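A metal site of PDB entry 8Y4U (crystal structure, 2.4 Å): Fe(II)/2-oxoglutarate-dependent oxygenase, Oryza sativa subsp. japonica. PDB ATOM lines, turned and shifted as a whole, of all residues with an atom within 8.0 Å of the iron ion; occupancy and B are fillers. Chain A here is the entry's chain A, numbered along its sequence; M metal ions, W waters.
The iron ion is bound by a ring nitrogen (NE2) of His 283 (2.0 Å), a ring nitrogen (NE2) of His 226 (2.1 Å) and the side-chain carboxylate (OD1) of Asp 228 (2.1 Å). Slightly farther from the iron ion lies water W2 (2.7 Å). Slightly farther from the iron ion lies water W1 (2.8 Å).
The side-chain amide nitrogen (ND2) of Asn 265 lies within hydrogen-bond range of the side-chain carboxylate (OD2) of Asp 228, at 3.4 Å. ND1 of His 226 sits at hydrogen-bond distance from O of Arg 224 (3.0 Å). A ring nitrogen (ND1) of His 283 is in hydrogen-bond range of the backbone carbonyl oxygen of Pro 281, at 3.1 Å. The side-chain hydroxyl (OG1) of Thr 233 is in hydrogen-bond range of the side-chain carboxylate (OD2) of Asp 228, at 2.8 Å.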
ATOM      1  N   PHE A  74       5.075  22.023  16.305  1.00  0.00           N
ATOM      2  CA  PHE A  74       6.053  20.961  16.128  1.00  0.00           C
ATOM      3  C   PHE A  74       6.415  20.365  17.466  1.00  0.00           C
ATOM      4  O   PHE A  74       6.345  21.034  18.499  1.00  0.00           O
ATOM      5  CB  PHE A  74       7.340  21.478  15.488  1.00  0.00           C
ATOM      6  CG  PHE A  74       7.229  21.724  14.033  1.00  0.00           C
ATOM      7  CD1 PHE A  74       6.787  22.936  13.567  1.00  0.00           C
ATOM      8  CD2 PHE A  74       7.570  20.739  13.130  1.00  0.00           C
ATOM      9  CE1 PHE A  74       6.680  23.162  12.218  1.00  0.00           C
ATOM     10  CE2 PHE A  74       7.466  20.974  11.783  1.00  0.00           C
ATOM     11  CZ  PHE A  74       7.030  22.181  11.330  1.00  0.00           C
ATOM     12  N   ARG A 207       9.256  12.228   0.924  1.00  0.00           N
ATOM     13  CA  ARG A 207       9.903  13.386   0.321  1.00  0.00           C
ATOM     14  C   ARG A 207      11.329  13.475   0.842  1.00  0.00           C
ATOM     15  O   ARG A 207      11.545  13.811   2.008  1.00  0.00           O
ATOM     16  CB  ARG A 207       9.123  14.660   0.621  1.00  0.00           C
ATOM     17  CG  ARG A 207       9.691  15.915   0.014  1.00  0.00           C
ATOM     18  CD  ARG A 207       8.833  17.089   0.422  1.00  0.00           C
ATOM     19  NE  ARG A 207       9.519  18.376   0.420  1.00  0.00           N
ATOM     20  CZ  ARG A 207       9.286  19.364  -0.440  1.00  0.00           C
ATOM     21  NH1 ARG A 207       8.374  19.236  -1.402  1.00  0.00           N
ATOM     22  NH2 ARG A 207       9.966  20.489  -0.327  1.00  0.00           N
ATOM     23  N   ILE A 223      13.268  26.633   1.328  1.00  0.00           N
ATOM     24  CA  ILE A 223      11.840  26.343   1.380  1.00  0.00           C
ATOM     25  C   ILE A 223      11.095  27.520   2.022  1.00  0.00           C
ATOM     26  O   ILE A 223      11.371  27.896   3.162  1.00  0.00           O
ATOM     27  CB  ILE A 223      11.578  25.038   2.145  1.00  0.00           C
ATOM     28  CG1 ILE A 223      12.576  23.967   1.695  1.00  0.00           C
ATOM     29  CG2 ILE A 223      10.135  24.557   1.950  1.00  0.00           C
ATOM     30  CD1 ILE A 223      12.511  23.643   0.199  1.00  0.00           C
ATOM     31  N   ARG A 224      10.172  28.107   1.284  1.00  0.00           N
ATOM     32  CA  ARG A 224       9.510  29.316   1.736  1.00  0.00           C
ATOM     33  C   ARG A 224       8.357  29.017   2.681  1.00  0.00           C
ATOM     34  O   ARG A 224       7.870  27.881   2.743  1.00  0.00           O
ATOM     35  CB  ARG A 224       9.039  30.105   0.525  1.00  0.00           C
ATOM     36  CG  ARG A 224      10.207  30.625  -0.244  1.00  0.00           C
ATOM     37  CD  ARG A 224       9.811  31.607  -1.293  1.00  0.00           C
ATOM     38  NE  ARG A 224      10.991  32.095  -1.998  1.00  0.00           N
ATOM     39  CZ  ARG A 224      10.951  33.023  -2.947  1.00  0.00           C
ATOM     40  NH1 ARG A 224       9.799  33.567  -3.291  1.00  0.00           N
ATOM     41  NH2 ARG A 224      12.078  33.399  -3.536  1.00  0.00           N
ATOM     42  N   PRO A 225       7.926  30.002   3.465  1.00  0.00           N
ATOM     43  CA  PRO A 225       6.870  29.789   4.446  1.00  0.00           C
ATOM     44  C   PRO A 225       5.661  29.085   3.855  1.00  0.00           C
ATOM     45  O   PRO A 225       5.216  29.412   2.761  1.00  0.00           O
ATOM     46  CB  PRO A 225       6.533  31.190   4.914  1.00  0.00           C
ATOM     47  CG  PRO A 225       7.841  31.912   4.825  1.00  0.00           C
ATOM     48  CD  PRO A 225       8.503  31.360   3.594  1.00  0.00           C
ATOM     49  N   HIS A 226       5.161  28.110   4.589  1.00  0.00           N
ATOM     50  CA  HIS A 226       4.040  27.322   4.104  1.00  0.00           C
ATOM     51  C   HIS A 226       3.499  26.518   5.277  1.00  0.00           C
ATOM     52  O   HIS A 226       4.178  26.315   6.280  1.00  0.00           O
ATOM     53  CB  HIS A 226       4.481  26.368   2.995  1.00  0.00           C
ATOM     54  CG  HIS A 226       5.306  25.235   3.483  1.00  0.00           C
ATOM     55  ND1 HIS A 226       6.655  25.351   3.733  1.00  0.00           N
ATOM     56  CD2 HIS A 226       4.960  23.968   3.826  1.00  0.00           C
ATOM     57  CE1 HIS A 226       7.115  24.191   4.180  1.00  0.00           C
ATOM     58  NE2 HIS A 226       6.106  23.339   4.253  1.00  0.00           N
ATOM     59  N   SER A 227       2.267  26.070   5.153  1.00  0.00           N
ATOM     60  CA  SER A 227       1.753  25.030   6.024  1.00  0.00           C
ATOM     61  C   SER A 227       1.638  23.753   5.205  1.00  0.00           C
ATOM     62  O   SER A 227       1.457  23.805   3.987  1.00  0.00           O
ATOM     63  CB  SER A 227       0.403  25.441   6.630  1.00  0.00           C
ATOM     64  OG  SER A 227      -0.528  25.785   5.620  1.00  0.00           O
ATOM     65  N   ASP A 228       1.806  22.614   5.859  1.00  0.00           N
ATOM     66  CA  ASP A 228       1.642  21.350   5.142  1.00  0.00           C
ATOM     67  C   ASP A 228       0.160  21.036   4.956  1.00  0.00           C
ATOM     68  O   ASP A 228      -0.669  21.348   5.802  1.00  0.00           O
ATOM     69  CB  ASP A 228       2.301  20.198   5.888  1.00  0.00           C
ATOM     70  CG  ASP A 228       3.833  20.287   5.944  1.00  0.00           C
ATOM     71  OD1 ASP A 228       4.451  21.189   5.349  1.00  0.00           O
ATOM     72  OD2 ASP A 228       4.423  19.419   6.597  1.00  0.00           O
ATOM     73  N   GLY A 229      -0.149  20.365   3.849  1.00  0.00           N
ATOM     74  CA  GLY A 229      -1.506  19.918   3.572  1.00  0.00           C
ATOM     75  C   GLY A 229      -1.896  18.581   4.147  1.00  0.00           C
ATOM     76  O   GLY A 229      -3.057  18.170   4.032  1.00  0.00           O
ATOM     77  N   THR A 230      -0.954  17.910   4.805  1.00  0.00           N
ATOM     78  CA  THR A 230      -1.095  16.536   5.251  1.00  0.00           C
ATOM     79  C   THR A 230      -2.045  16.429   6.424  1.00  0.00           C
ATOM     80  O   THR A 230      -2.493  17.412   6.998  1.00  0.00           O
ATOM     81  CB  THR A 230       0.254  15.982   5.687  1.00  0.00           C
ATOM     82  OG1 THR A 230       0.732  16.767   6.785  1.00  0.00           O
ATOM     83  CG2 THR A 230       1.231  16.055   4.561  1.00  0.00           C
ATOM     84  N   THR A 233       2.885  14.936   9.420  1.00  0.00           N
ATOM     85  CA  THR A 233       4.189  14.963   8.771  1.00  0.00           C
ATOM     86  C   THR A 233       5.235  14.459   9.759  1.00  0.00           C
ATOM     87  O   THR A 233       5.303  14.948  10.893  1.00  0.00           O
ATOM     88  CB  THR A 233       4.547  16.371   8.302  1.00  0.00           C
ATOM     89  OG1 THR A 233       3.671  16.753   7.242  1.00  0.00           O
ATOM     90  CG2 THR A 233       5.995  16.444   7.810  1.00  0.00           C
ATOM     91  N   LEU A 235       9.296  13.968  10.043  1.00  0.00           N
ATOM     92  CA  LEU A 235      10.523  14.445   9.429  1.00  0.00           C
ATOM     93  C   LEU A 235      11.755  13.854  10.119  1.00  0.00           C
ATOM     94  O   LEU A 235      11.839  13.846  11.350  1.00  0.00           O
ATOM     95  CB  LEU A 235      10.592  15.970   9.494  1.00  0.00           C
ATOM     96  CG  LEU A 235      11.778  16.644   8.785  1.00  0.00           C
ATOM     97  CD1 LEU A 235      11.676  16.572   7.267  1.00  0.00           C
ATOM     98  CD2 LEU A 235      11.917  18.071   9.226  1.00  0.00           C
ATOM     99  N   LEU A 244      15.189  24.207   9.752  1.00  0.00           N
ATOM    100  CA  LEU A 244      13.739  24.245   9.884  1.00  0.00           C
ATOM    101  C   LEU A 244      13.328  25.286  10.919  1.00  0.00           C
ATOM    102  O   LEU A 244      13.864  25.317  12.031  1.00  0.00           O
ATOM    103  CB  LEU A 244      13.217  22.861  10.254  1.00  0.00           C
ATOM    104  CG  LEU A 244      11.722  22.714  10.558  1.00  0.00           C
ATOM    105  CD1 LEU A 244      10.844  23.078   9.366  1.00  0.00           C
ATOM    106  CD2 LEU A 244      11.416  21.328  11.039  1.00  0.00           C
ATOM    107  N   ASN A 265       4.738  17.365  12.995  1.00  0.00           N
ATOM    108  CA  ASN A 265       3.767  18.428  12.960  1.00  0.00           C
ATOM    109  C   ASN A 265       2.495  17.882  12.325  1.00  0.00           C
ATOM    110  O   ASN A 265       2.518  16.945  11.528  1.00  0.00           O
ATOM    111  CB  ASN A 265       4.275  19.642  12.186  1.00  0.00           C
ATOM    112  CG  ASN A 265       4.560  19.339  10.735  1.00  0.00           C
ATOM    113  OD1 ASN A 265       5.602  18.797  10.385  1.00  0.00           O
ATOM    114  ND2 ASN A 265       3.649  19.739   9.857  1.00  0.00           N
ATOM    115  N   PRO A 281       1.108  24.365  11.675  1.00  0.00           N
ATOM    116  CA  PRO A 281       2.044  25.487  11.806  1.00  0.00           C
ATOM    117  C   PRO A 281       2.631  25.942  10.473  1.00  0.00           C
ATOM    118  O   PRO A 281       2.928  25.145   9.591  1.00  0.00           O
ATOM    119  CB  PRO A 281       3.140  24.911  12.705  1.00  0.00           C
ATOM    120  CG  PRO A 281       3.138  23.457  12.375  1.00  0.00           C
ATOM    121  CD  PRO A 281       1.684  23.116  12.206  1.00  0.00           C
ATOM    122  N   VAL A 282       2.800  27.238  10.348  1.00  0.00           N
ATOM    123  CA  VAL A 282       3.538  27.801   9.214  1.00  0.00           C
ATOM    124  C   VAL A 282       5.025  27.630   9.474  1.00  0.00           C
ATOM    125  O   VAL A 282       5.509  27.914  10.581  1.00  0.00           O
ATOM    126  CB  VAL A 282       3.147  29.266   9.006  1.00  0.00           C
ATOM    127  CG1 VAL A 282       4.016  29.945   7.957  1.00  0.00           C
ATOM    128  CG2 VAL A 282       1.681  29.338   8.600  1.00  0.00           C
ATOM    129  N   HIS A 283       5.750  27.106   8.496  1.00  0.00           N
ATOM    130  CA  HIS A 283       7.162  26.820   8.714  1.00  0.00           C
ATOM    131  C   HIS A 283       7.945  27.064   7.434  1.00  0.00           C
ATOM    132  O   HIS A 283       7.379  27.297   6.369  1.00  0.00           O
ATOM    133  CB  HIS A 283       7.355  25.407   9.243  1.00  0.00           C
ATOM    134  CG  HIS A 283       6.809  24.337   8.349  1.00  0.00           C
ATOM    135  ND1 HIS A 283       5.483  23.958   8.383  1.00  0.00           N
ATOM    136  CD2 HIS A 283       7.411  23.527   7.458  1.00  0.00           C
ATOM    137  CE1 HIS A 283       5.288  22.977   7.521  1.00  0.00           C
ATOM    138  NE2 HIS A 283       6.440  22.699   6.947  1.00  0.00           N
ATOM    139  N   ARG A 284       9.271  27.024   7.557  1.00  0.00           N
ATOM    140  CA  ARG A 284      10.160  27.245   6.419  1.00  0.00           C
ATOM    141  C   ARG A 284      11.498  26.578   6.718  1.00  0.00           C
ATOM    142  O   ARG A 284      11.809  26.273   7.873  1.00  0.00           O
ATOM    143  CB  ARG A 284      10.341  28.743   6.145  1.00  0.00           C
ATOM    144  CG  ARG A 284      11.199  29.460   7.169  1.00  0.00           C
ATOM    145  CD  ARG A 284      11.328  30.961   6.919  1.00  0.00           C
ATOM    146  NE  ARG A 284      12.162  31.577   7.941  1.00  0.00           N
ATOM    147  CZ  ARG A 284      12.224  32.872   8.207  1.00  0.00           C
ATOM    148  NH1 ARG A 284      11.477  33.729   7.527  1.00  0.00           N
ATOM    149  NH2 ARG A 284      13.026  33.307   9.171  1.00  0.00           N
ATOM    150  N   VAL A 285      12.289  26.324   5.672  1.00  0.00           N
ATOM    151  CA  VAL A 285      13.590  25.671   5.809  1.00  0.00           C
ATOM    152  C   VAL A 285      14.618  26.571   5.138  1.00  0.00           C
ATOM    153  O   VAL A 285      14.744  26.587   3.909  1.00  0.00           O
ATOM    154  CB  VAL A 285      13.636  24.264   5.202  1.00  0.00           C
ATOM    155  CG1 VAL A 285      15.034  23.673   5.340  1.00  0.00           C
ATOM    156  CG2 VAL A 285      12.619  23.353   5.854  1.00  0.00           C
ATOM    157  N   ALA A 297      10.910  13.571   4.706  1.00  0.00           N
ATOM    158  CA  ALA A 297       9.595  13.798   5.289  1.00  0.00           C
ATOM    159  C   ALA A 297       8.655  12.687   4.846  1.00  0.00           C
ATOM    160  O   ALA A 297       8.548  12.402   3.663  1.00  0.00           O
ATOM    161  CB  ALA A 297       9.029  15.160   4.895  1.00  0.00           C
ATOM    162  N   LEU A 299       4.859  11.957   4.500  1.00  0.00           N
ATOM    163  CA  LEU A 299       3.700  12.836   4.350  1.00  0.00           C
ATOM    164  C   LEU A 299       2.428  11.982   4.305  1.00  0.00           C
ATOM    165  O   LEU A 299       2.178  11.291   3.314  1.00  0.00           O
ATOM    166  CB  LEU A 299       3.845  13.683   3.082  1.00  0.00           C
ATOM    167  CG  LEU A 299       5.131  14.511   2.999  1.00  0.00           C
ATOM    168  CD1 LEU A 299       5.324  15.056   1.600  1.00  0.00           C
ATOM    169  CD2 LEU A 299       5.166  15.634   4.004  1.00  0.00           C
HETATM  170 FE    FE M   1       6.521  21.617   5.314  1.00  0.00          FE
HETATM  171  O   HOH W   1       9.152  21.616   4.308  1.00  0.00           O
HETATM  172  O   HOH W   2       7.140  18.988   5.026  1.00  0.00           O
